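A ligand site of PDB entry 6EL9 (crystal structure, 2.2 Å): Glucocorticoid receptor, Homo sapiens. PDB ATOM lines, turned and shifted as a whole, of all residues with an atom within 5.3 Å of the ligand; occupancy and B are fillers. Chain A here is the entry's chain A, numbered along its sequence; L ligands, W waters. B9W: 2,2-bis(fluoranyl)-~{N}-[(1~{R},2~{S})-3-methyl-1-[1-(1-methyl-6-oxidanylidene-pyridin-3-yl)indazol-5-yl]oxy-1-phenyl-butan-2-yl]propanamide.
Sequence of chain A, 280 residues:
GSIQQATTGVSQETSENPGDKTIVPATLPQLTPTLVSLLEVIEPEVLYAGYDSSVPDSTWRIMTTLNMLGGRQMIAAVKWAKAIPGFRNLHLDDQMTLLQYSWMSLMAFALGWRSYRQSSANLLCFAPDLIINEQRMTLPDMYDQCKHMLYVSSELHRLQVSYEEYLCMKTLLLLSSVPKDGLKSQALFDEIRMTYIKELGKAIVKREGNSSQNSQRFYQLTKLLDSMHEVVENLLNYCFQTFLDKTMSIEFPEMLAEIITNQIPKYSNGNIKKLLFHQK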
ATOM      1  N   MET A  63     -20.007  29.233 -10.442  1.00  0.00           N
ATOM      2  CA  MET A  63     -19.693  30.273  -9.468  1.00  0.00           C
ATOM      3  C   MET A  63     -20.895  31.153  -9.160  1.00  0.00           C
ATOM      4  O   MET A  63     -21.119  31.480  -8.006  1.00  0.00           O
ATOM      5  CB  MET A  63     -18.527  31.124  -9.949  1.00  0.00           C
ATOM      6  CG  MET A  63     -17.161  30.502  -9.741  1.00  0.00           C
ATOM      7  SD  MET A  63     -15.857  31.548 -10.485  1.00  0.00           S
ATOM      8  CE  MET A  63     -15.776  32.922  -9.286  1.00  0.00           C
ATOM      9  N   LEU A  66     -23.585  29.063  -7.244  1.00  0.00           N
ATOM     10  CA  LEU A  66     -23.092  28.849  -5.874  1.00  0.00           C
ATOM     11  C   LEU A  66     -23.155  30.105  -5.000  1.00  0.00           C
ATOM     12  O   LEU A  66     -23.359  29.983  -3.799  1.00  0.00           O
ATOM     13  CB  LEU A  66     -21.675  28.239  -5.871  1.00  0.00           C
ATOM     14  CG  LEU A  66     -21.571  26.811  -6.434  1.00  0.00           C
ATOM     15  CD1 LEU A  66     -20.154  26.294  -6.370  1.00  0.00           C
ATOM     16  CD2 LEU A  66     -22.470  25.871  -5.675  1.00  0.00           C
ATOM     17  N   ASN A  67     -23.007  31.297  -5.597  1.00  0.00           N
ATOM     18  CA  ASN A  67     -23.133  32.561  -4.872  1.00  0.00           C
ATOM     19  C   ASN A  67     -24.583  32.773  -4.460  1.00  0.00           C
ATOM     20  O   ASN A  67     -24.835  33.135  -3.310  1.00  0.00           O
ATOM     21  CB  ASN A  67     -22.634  33.753  -5.698  1.00  0.00           C
ATOM     22  CG  ASN A  67     -21.162  33.950  -5.651  1.00  0.00           C
ATOM     23  OD1 ASN A  67     -20.456  33.266  -4.908  1.00  0.00           O
ATOM     24  ND2 ASN A  67     -20.645  34.848  -6.469  1.00  0.00           N
ATOM     25  N   LEU A  69     -26.871  30.356  -4.080  1.00  0.00           N
ATOM     26  CA  LEU A  69     -27.113  29.301  -3.082  1.00  0.00           C
ATOM     27  C   LEU A  69     -26.524  29.707  -1.734  1.00  0.00           C
ATOM     28  O   LEU A  69     -27.181  29.549  -0.705  1.00  0.00           O
ATOM     29  CB  LEU A  69     -26.531  27.935  -3.571  1.00  0.00           C
ATOM     30  CG  LEU A  69     -26.599  26.737  -2.576  1.00  0.00           C
ATOM     31  CD1 LEU A  69     -28.059  26.313  -2.238  1.00  0.00           C
ATOM     32  CD2 LEU A  69     -25.766  25.555  -3.101  1.00  0.00           C
ATOM     33  N   GLY A  70     -25.301  30.261  -1.755  1.00  0.00           N
ATOM     34  CA  GLY A  70     -24.596  30.746  -0.568  1.00  0.00           C
ATOM     35  C   GLY A  70     -25.379  31.796   0.213  1.00  0.00           C
ATOM     36  O   GLY A  70     -25.355  31.789   1.433  1.00  0.00           O
ATOM     37  N   GLN A  73     -28.175  29.866   2.008  1.00  0.00           N
ATOM     38  CA  GLN A  73     -27.514  29.134   3.091  1.00  0.00           C
ATOM     39  C   GLN A  73     -27.190  30.103   4.244  1.00  0.00           C
ATOM     40  O   GLN A  73     -27.363  29.719   5.395  1.00  0.00           O
ATOM     41  CB  GLN A  73     -26.205  28.478   2.604  1.00  0.00           C
ATOM     42  CG  GLN A  73     -26.345  27.551   1.395  1.00  0.00           C
ATOM     43  CD  GLN A  73     -26.652  26.113   1.707  1.00  0.00           C
ATOM     44  OE1 GLN A  73     -27.348  25.783   2.664  1.00  0.00           O
ATOM     45  NE2 GLN A  73     -26.175  25.223   0.845  1.00  0.00           N
ATOM     46  N   TRP A 103     -19.139  33.818   8.922  1.00  0.00           N
ATOM     47  CA  TRP A 103     -19.989  33.326   7.835  1.00  0.00           C
ATOM     48  C   TRP A 103     -19.281  32.313   6.900  1.00  0.00           C
ATOM     49  O   TRP A 103     -19.820  31.227   6.680  1.00  0.00           O
ATOM     50  CB  TRP A 103     -20.596  34.504   7.051  1.00  0.00           C
ATOM     51  CG  TRP A 103     -19.644  35.235   6.160  1.00  0.00           C
ATOM     52  CD1 TRP A 103     -18.707  36.140   6.540  1.00  0.00           C
ATOM     53  CD2 TRP A 103     -19.509  35.082   4.743  1.00  0.00           C
ATOM     54  NE1 TRP A 103     -17.992  36.561   5.446  1.00  0.00           N
ATOM     55  CE2 TRP A 103     -18.507  35.964   4.322  1.00  0.00           C
ATOM     56  CE3 TRP A 103     -20.151  34.277   3.789  1.00  0.00           C
ATOM     57  CZ2 TRP A 103     -18.125  36.074   2.977  1.00  0.00           C
ATOM     58  CZ3 TRP A 103     -19.772  34.392   2.460  1.00  0.00           C
ATOM     59  CH2 TRP A 103     -18.787  35.293   2.067  1.00  0.00           C
ATOM     60  N   MET A 104     -18.079  32.640   6.402  1.00  0.00           N
ATOM     61  CA  MET A 104     -17.324  31.782   5.491  1.00  0.00           C
ATOM     62  C   MET A 104     -16.838  30.497   6.179  1.00  0.00           C
ATOM     63  O   MET A 104     -16.855  29.445   5.532  1.00  0.00           O
ATOM     64  CB  MET A 104     -16.175  32.551   4.769  1.00  0.00           C
ATOM     65  CG  MET A 104     -15.448  31.732   3.687  1.00  0.00           C
ATOM     66  SD  MET A 104     -16.488  31.141   2.304  1.00  0.00           S
ATOM     67  CE  MET A 104     -16.283  32.518   1.175  1.00  0.00           C
ATOM     68  N   LEU A 106     -18.359  28.937   8.700  1.00  0.00           N
ATOM     69  CA  LEU A 106     -19.581  28.159   8.852  1.00  0.00           C
ATOM     70  C   LEU A 106     -19.959  27.486   7.518  1.00  0.00           C
ATOM     71  O   LEU A 106     -20.183  26.277   7.491  1.00  0.00           O
ATOM     72  CB  LEU A 106     -20.750  29.026   9.367  1.00  0.00           C
ATOM     73  CG  LEU A 106     -20.573  29.709  10.743  1.00  0.00           C
ATOM     74  CD1 LEU A 106     -21.754  30.642  11.013  1.00  0.00           C
ATOM     75  CD2 LEU A 106     -20.427  28.687  11.877  1.00  0.00           C
ATOM     76  N   MET A 107     -19.932  28.258   6.404  1.00  0.00           N
ATOM     77  CA  MET A 107     -20.255  27.766   5.057  1.00  0.00           C
ATOM     78  C   MET A 107     -19.305  26.639   4.651  1.00  0.00           C
ATOM     79  O   MET A 107     -19.769  25.583   4.230  1.00  0.00           O
ATOM     80  CB  MET A 107     -20.188  28.892   3.999  1.00  0.00           C
ATOM     81  CG  MET A 107     -21.143  30.057   4.225  1.00  0.00           C
ATOM     82  SD  MET A 107     -22.848  29.728   3.787  1.00  0.00           S
ATOM     83  CE  MET A 107     -23.488  29.225   5.347  1.00  0.00           C
ATOM     84  N   ALA A 108     -17.979  26.879   4.739  1.00  0.00           N
ATOM     85  CA  ALA A 108     -16.946  25.908   4.363  1.00  0.00           C
ATOM     86  C   ALA A 108     -16.987  24.655   5.239  1.00  0.00           C
ATOM     87  O   ALA A 108     -16.769  23.542   4.733  1.00  0.00           O
ATOM     88  CB  ALA A 108     -15.562  26.550   4.402  1.00  0.00           C
ATOM     89  N   ALA A 110     -19.717  23.450   6.991  1.00  0.00           N
ATOM     90  CA  ALA A 110     -20.959  22.729   6.682  1.00  0.00           C
ATOM     91  C   ALA A 110     -20.849  22.002   5.339  1.00  0.00           C
ATOM     92  O   ALA A 110     -21.262  20.864   5.238  1.00  0.00           O
ATOM     93  CB  ALA A 110     -22.156  23.656   6.717  1.00  0.00           C
ATOM     94  N   LEU A 111     -20.176  22.643   4.350  1.00  0.00           N
ATOM     95  CA  LEU A 111     -19.911  22.044   3.041  1.00  0.00           C
ATOM     96  C   LEU A 111     -18.957  20.832   3.169  1.00  0.00           C
ATOM     97  O   LEU A 111     -19.227  19.810   2.542  1.00  0.00           O
ATOM     98  CB  LEU A 111     -19.345  23.095   2.064  1.00  0.00           C
ATOM     99  CG  LEU A 111     -18.756  22.580   0.740  1.00  0.00           C
ATOM    100  CD1 LEU A 111     -19.846  22.082  -0.183  1.00  0.00           C
ATOM    101  CD2 LEU A 111     -17.951  23.660   0.059  1.00  0.00           C
ATOM    102  N   ARG A 114     -20.985  17.912   4.611  1.00  0.00           N
ATOM    103  CA  ARG A 114     -21.892  17.339   3.615  1.00  0.00           C
ATOM    104  C   ARG A 114     -21.151  16.539   2.559  1.00  0.00           C
ATOM    105  O   ARG A 114     -21.675  15.529   2.095  1.00  0.00           O
ATOM    106  CB  ARG A 114     -22.859  18.367   2.984  1.00  0.00           C
ATOM    107  CG  ARG A 114     -24.197  17.670   2.738  1.00  0.00           C
ATOM    108  CD  ARG A 114     -25.362  18.543   2.383  1.00  0.00           C
ATOM    109  NE  ARG A 114     -25.848  19.315   3.529  1.00  0.00           N
ATOM    110  CZ  ARG A 114     -26.719  20.297   3.423  1.00  0.00           C
ATOM    111  NH1 ARG A 114     -27.112  20.969   4.501  1.00  0.00           N
ATOM    112  NH2 ARG A 114     -27.213  20.634   2.240  1.00  0.00           N
ATOM    113  N   CYS A 125     -19.915  18.553  -2.282  1.00  0.00           N
ATOM    114  CA  CYS A 125     -21.357  18.423  -2.364  1.00  0.00           C
ATOM    115  C   CYS A 125     -22.013  19.702  -1.866  1.00  0.00           C
ATOM    116  O   CYS A 125     -22.435  19.786  -0.709  1.00  0.00           O
ATOM    117  CB  CYS A 125     -21.841  17.181  -1.618  1.00  0.00           C
ATOM    118  SG  CYS A 125     -20.974  15.653  -2.090  1.00  0.00           S
ATOM    119  N   PHE A 126     -22.053  20.725  -2.741  1.00  0.00           N
ATOM    120  CA  PHE A 126     -22.660  22.018  -2.417  1.00  0.00           C
ATOM    121  C   PHE A 126     -24.133  21.890  -2.204  1.00  0.00           C
ATOM    122  O   PHE A 126     -24.693  22.528  -1.310  1.00  0.00           O
ATOM    123  CB  PHE A 126     -22.388  23.026  -3.523  1.00  0.00           C
ATOM    124  CG  PHE A 126     -20.990  23.591  -3.506  1.00  0.00           C
ATOM    125  CD1 PHE A 126     -20.693  24.707  -2.745  1.00  0.00           C
ATOM    126  CD2 PHE A 126     -19.993  23.021  -4.285  1.00  0.00           C
ATOM    127  CE1 PHE A 126     -19.406  25.245  -2.744  1.00  0.00           C
ATOM    128  CE2 PHE A 126     -18.703  23.576  -4.302  1.00  0.00           C
ATOM    129  CZ  PHE A 126     -18.415  24.671  -3.517  1.00  0.00           C
ATOM    130  N   ALA A 127     -24.776  21.048  -3.028  1.00  0.00           N
ATOM    131  CA  ALA A 127     -26.213  20.770  -3.018  1.00  0.00           C
ATOM    132  C   ALA A 127     -26.395  19.405  -3.646  1.00  0.00           C
ATOM    133  O   ALA A 127     -25.515  18.989  -4.422  1.00  0.00           O
ATOM    134  CB  ALA A 127     -26.942  21.834  -3.842  1.00  0.00           C
ATOM    135  N   GLN A 145     -10.006  27.252  -6.604  1.00  0.00           N
ATOM    136  CA  GLN A 145     -10.970  27.748  -5.640  1.00  0.00           C
ATOM    137  C   GLN A 145     -11.562  26.599  -4.783  1.00  0.00           C
ATOM    138  O   GLN A 145     -11.737  26.765  -3.580  1.00  0.00           O
ATOM    139  CB  GLN A 145     -12.044  28.643  -6.295  1.00  0.00           C
ATOM    140  CG  GLN A 145     -12.741  28.080  -7.511  1.00  0.00           C
ATOM    141  CD  GLN A 145     -13.613  29.119  -8.165  1.00  0.00           C
ATOM    142  OE1 GLN A 145     -14.736  29.382  -7.725  1.00  0.00           O
ATOM    143  NE2 GLN A 145     -13.109  29.738  -9.226  1.00  0.00           N
ATOM    144  N   MET A 149     -11.650  24.127   0.099  1.00  0.00           N
ATOM    145  CA  MET A 149     -12.860  23.492   0.618  1.00  0.00           C
ATOM    146  C   MET A 149     -12.645  21.997   0.706  1.00  0.00           C
ATOM    147  O   MET A 149     -13.042  21.386   1.690  1.00  0.00           O
ATOM    148  CB  MET A 149     -14.073  23.846  -0.232  1.00  0.00           C
ATOM    149  CG  MET A 149     -14.578  25.238   0.040  1.00  0.00           C
ATOM    150  SD  MET A 149     -15.585  25.956  -1.266  1.00  0.00           S
ATOM    151  CE  MET A 149     -14.621  25.662  -2.666  1.00  0.00           C
ATOM    152  N   LEU A 235     -10.167  31.473   0.981  1.00  0.00           N
ATOM    153  CA  LEU A 235     -11.475  31.590   0.328  1.00  0.00           C
ATOM    154  C   LEU A 235     -11.925  33.049   0.205  1.00  0.00           C
ATOM    155  O   LEU A 235     -12.550  33.406  -0.797  1.00  0.00           O
ATOM    156  CB  LEU A 235     -12.565  30.783   1.066  1.00  0.00           C
ATOM    157  CG  LEU A 235     -12.419  29.260   1.084  1.00  0.00           C
ATOM    158  CD1 LEU A 235     -13.364  28.660   2.069  1.00  0.00           C
ATOM    159  CD2 LEU A 235     -12.578  28.657  -0.315  1.00  0.00           C
ATOM    160  N   TYR A 238     -10.248  35.047  -2.785  1.00  0.00           N
ATOM    161  CA  TYR A 238     -10.977  34.781  -4.038  1.00  0.00           C
ATOM    162  C   TYR A 238     -12.288  35.589  -4.007  1.00  0.00           C
ATOM    163  O   TYR A 238     -12.623  36.279  -4.972  1.00  0.00           O
ATOM    164  CB  TYR A 238     -11.359  33.292  -4.110  1.00  0.00           C
ATOM    165  CG  TYR A 238     -10.660  32.507  -5.196  1.00  0.00           C
ATOM    166  CD1 TYR A 238     -11.119  32.541  -6.513  1.00  0.00           C
ATOM    167  CD2 TYR A 238      -9.604  31.650  -4.890  1.00  0.00           C
ATOM    168  CE1 TYR A 238     -10.475  31.814  -7.523  1.00  0.00           C
ATOM    169  CE2 TYR A 238      -8.959  30.919  -5.886  1.00  0.00           C
ATOM    170  CZ  TYR A 238      -9.399  31.003  -7.198  1.00  0.00           C
ATOM    171  OH  TYR A 238      -8.777  30.271  -8.186  1.00  0.00           O
ATOM    172  N   CYS A 239     -13.027  35.492  -2.877  1.00  0.00           N
ATOM    173  CA  CYS A 239     -14.302  36.152  -2.631  1.00  0.00           C
ATOM    174  C   CYS A 239     -14.245  37.695  -2.793  1.00  0.00           C
ATOM    175  O   CYS A 239     -15.053  38.247  -3.522  1.00  0.00           O
ATOM    176  CB  CYS A 239     -14.863  35.750  -1.283  1.00  0.00           C
ATOM    177  SG  CYS A 239     -16.408  36.566  -0.858  1.00  0.00           S
ATOM    178  N   THR A 242     -13.226  38.728  -6.471  1.00  0.00           N
ATOM    179  CA  THR A 242     -14.369  38.428  -7.346  1.00  0.00           C
ATOM    180  C   THR A 242     -15.503  39.445  -7.115  1.00  0.00           C
ATOM    181  O   THR A 242     -16.191  39.844  -8.074  1.00  0.00           O
ATOM    182  CB  THR A 242     -14.756  36.937  -7.148  1.00  0.00           C
ATOM    183  OG1 THR A 242     -13.844  36.121  -7.879  1.00  0.00           O
ATOM    184  CG2 THR A 242     -16.124  36.616  -7.592  1.00  0.00           C
ATOM    185  N   ILE A 250     -19.666  38.774 -11.827  1.00  0.00           N
ATOM    186  CA  ILE A 250     -20.010  37.736 -10.871  1.00  0.00           C
ATOM    187  C   ILE A 250     -21.023  38.344  -9.898  1.00  0.00           C
ATOM    188  O   ILE A 250     -20.699  39.263  -9.147  1.00  0.00           O
ATOM    189  CB  ILE A 250     -18.789  37.110 -10.145  1.00  0.00           C
ATOM    190  CG1 ILE A 250     -17.765  36.453 -11.125  1.00  0.00           C
ATOM    191  CG2 ILE A 250     -19.247  36.136  -9.057  1.00  0.00           C
ATOM    192  CD1 ILE A 250     -18.136  35.089 -11.736  1.00  0.00           C
ATOM    193  N   PHE A 252     -23.455  38.539  -6.672  1.00  0.00           N
ATOM    194  CA  PHE A 252     -23.552  38.203  -5.277  1.00  0.00           C
ATOM    195  C   PHE A 252     -24.938  38.622  -4.805  1.00  0.00           C
ATOM    196  O   PHE A 252     -25.362  39.750  -5.091  1.00  0.00           O
ATOM    197  CB  PHE A 252     -22.484  38.915  -4.435  1.00  0.00           C
ATOM    198  CG  PHE A 252     -21.098  38.334  -4.614  1.00  0.00           C
ATOM    199  CD1 PHE A 252     -20.312  38.704  -5.703  1.00  0.00           C
ATOM    200  CD2 PHE A 252     -20.590  37.426  -3.701  1.00  0.00           C
ATOM    201  CE1 PHE A 252     -19.059  38.137  -5.879  1.00  0.00           C
ATOM    202  CE2 PHE A 252     -19.314  36.897  -3.860  1.00  0.00           C
ATOM    203  CZ  PHE A 252     -18.551  37.266  -4.942  1.00  0.00           C
ATOM    204  N   LEU A 256     -24.920  38.221   0.927  1.00  0.00           N
ATOM    205  CA  LEU A 256     -23.463  38.127   0.846  1.00  0.00           C
ATOM    206  C   LEU A 256     -22.823  39.461   0.527  1.00  0.00           C
ATOM    207  O   LEU A 256     -21.830  39.792   1.168  1.00  0.00           O
ATOM    208  CB  LEU A 256     -23.009  37.036  -0.157  1.00  0.00           C
ATOM    209  CG  LEU A 256     -23.540  35.619   0.091  1.00  0.00           C
ATOM    210  CD1 LEU A 256     -22.966  34.656  -0.927  1.00  0.00           C
ATOM    211  CD2 LEU A 256     -23.242  35.152   1.505  1.00  0.00           C
ATOM    212  N   ILE A 260     -19.866  41.112   2.833  1.00  0.00           N
ATOM    213  CA  ILE A 260     -18.576  41.409   2.169  1.00  0.00           C
ATOM    214  C   ILE A 260     -18.227  42.918   2.284  1.00  0.00           C
ATOM    215  O   ILE A 260     -17.100  43.253   2.627  1.00  0.00           O
ATOM    216  CB  ILE A 260     -18.519  40.862   0.708  1.00  0.00           C
ATOM    217  CG1 ILE A 260     -18.667  39.320   0.706  1.00  0.00           C
ATOM    218  CG2 ILE A 260     -17.214  41.265   0.005  1.00  0.00           C
ATOM    219  CD1 ILE A 260     -19.285  38.757  -0.558  1.00  0.00           C
HETATM  220  C1  B9W L   1     -20.176  32.341  -0.252  1.00  0.00           C
HETATM  221  C2  B9W L   1     -19.680  32.817  -1.600  1.00  0.00           C
HETATM  222  C3  B9W L   1     -19.206  34.239  -1.360  1.00  0.00           C
HETATM  223  N6  B9W L   1     -18.206  32.483  -3.534  1.00  0.00           N
HETATM  224  C7  B9W L   1     -16.958  33.016  -3.759  1.00  0.00           C
HETATM  225  C9  B9W L   1     -16.537  33.138  -5.212  1.00  0.00           C
HETATM  226  C10 B9W L   1     -16.251  31.765  -5.762  1.00  0.00           C
HETATM  227  C13 B9W L   1     -18.959  30.476  -2.334  1.00  0.00           C
HETATM  228  C16 B9W L   1     -19.744  28.932  -0.738  1.00  0.00           C
HETATM  229  C19 B9W L   1     -21.512  27.014   0.029  1.00  0.00           C
HETATM  230  C20 B9W L   1     -21.802  27.861  -1.035  1.00  0.00           C
HETATM  231  C21 B9W L   1     -23.055  27.439  -1.512  1.00  0.00           C
HETATM  232  N23 B9W L   1     -22.579  26.148   0.149  1.00  0.00           N
HETATM  233  C24 B9W L   1     -22.867  25.289   1.216  1.00  0.00           C
HETATM  234  N26 B9W L   1     -23.487  23.154   2.074  1.00  0.00           N
HETATM  235  C27 B9W L   1     -23.776  21.764   1.819  1.00  0.00           C
HETATM  236  C30 B9W L   1     -23.451  25.096   3.589  1.00  0.00           C
HETATM  237  C31 B9W L   1     -23.043  25.830   2.541  1.00  0.00           C
HETATM  238  C32 B9W L   1     -20.923  28.847  -1.444  1.00  0.00           C
HETATM  239  C33 B9W L   1     -18.087  29.715  -3.268  1.00  0.00           C
HETATM  240  C34 B9W L   1     -16.787  29.399  -2.939  1.00  0.00           C
HETATM  241  C35 B9W L   1     -16.014  28.674  -3.823  1.00  0.00           C
HETATM  242  C4  B9W L   1     -18.589  31.954  -2.235  1.00  0.00           C
HETATM  243  O8  B9W L   1     -16.209  33.378  -2.856  1.00  0.00           O
HETATM  244  F11 B9W L   1     -17.393  33.794  -6.058  1.00  0.00           F
HETATM  245  F12 B9W L   1     -15.379  33.831  -5.266  1.00  0.00           F
HETATM  246  O15 B9W L   1     -18.767  29.882  -1.044  1.00  0.00           O
HETATM  247  C17 B9W L   1     -19.475  28.097   0.330  1.00  0.00           C
HETATM  248  C18 B9W L   1     -20.343  27.103   0.744  1.00  0.00           C
HETATM  249  N22 B9W L   1     -23.500  26.420  -0.796  1.00  0.00           N
HETATM  250  C25 B9W L   1     -23.105  23.980   1.017  1.00  0.00           C
HETATM  251  C28 B9W L   1     -23.718  23.644   3.345  1.00  0.00           C
HETATM  252  O29 B9W L   1     -24.126  22.948   4.263  1.00  0.00           O
HETATM  253  C36 B9W L   1     -16.525  28.260  -5.037  1.00  0.00           C
HETATM  254  C37 B9W L   1     -17.825  28.598  -5.368  1.00  0.00           C
HETATM  255  C38 B9W L   1     -18.601  29.310  -4.480  1.00  0.00           C
HETATM  256  O   HOH W   1     -25.815  23.948   6.642  1.00  0.00           O
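The side-chain amide nitrogen of Gln 145 is in hydrogen-bond range of the side-chain sulfur of Met 63, 3.5 Å away.
The backbone carbonyl oxygen (O) of Tyr 238 sits close to the side-chain hydroxyl (OG1) of Thr 242 (3.2 Å).
A nitrogen (N22) of the ligand sits close to the side-chain amide nitrogen (NE2) of Gln 73 (3.4 Å).
A nitrogen (N6) of the ligand lies within hydrogen-bond range of the side-chain amide oxygen (OD1) of Asn 67 (2.8 Å).
An oxygen (O8) of the ligand sits close to the side-chain sulfur (SG) of Cys 239, 3.8 Å away.
Residues that only touch the ligand: Phe 126 (3.2 Å), Ala 110 (3.2 Å), Leu 69 (3.3 Å), Gln 145 (3.4 Å), Trp 103 (3.4 Å), Leu 66 (3.4 Å), Thr 242 (3.5 Å), Cys 125 (3.5 Å), Met 149 (3.5 Å), Arg 114 (3.6 Å), Gly 70 (3.6 Å), Phe 252 (3.7 Å), Leu 256 (3.7 Å), Met 107 (3.7 Å), Tyr 238 (3.7 Å), Met 63 (3.7 Å) and Leu 111 (3.8 Å).
Hydrophobic or aromatic side chains within 4 Å of the ligand: Met 63, Leu 66, Leu 69, Trp 103, Met 107, Ala 110, Leu 111, Phe 126, Met 149, Phe 252 and Leu 256.
20 residues have an atom within 4 Å of the ligand: Met 63, Leu 66, Asn 67, Leu 69, Gly 70, Gln 73, Trp 103, Met 107, Ala 110, Leu 111, Arg 114, Cys 125, Phe 126, Gln 145, Met 149, Tyr 238, Cys 239, Thr 242, Phe 252 and Leu 256.
Along chain A the residues within 4 Å of the ligand span positions 63 to 256.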
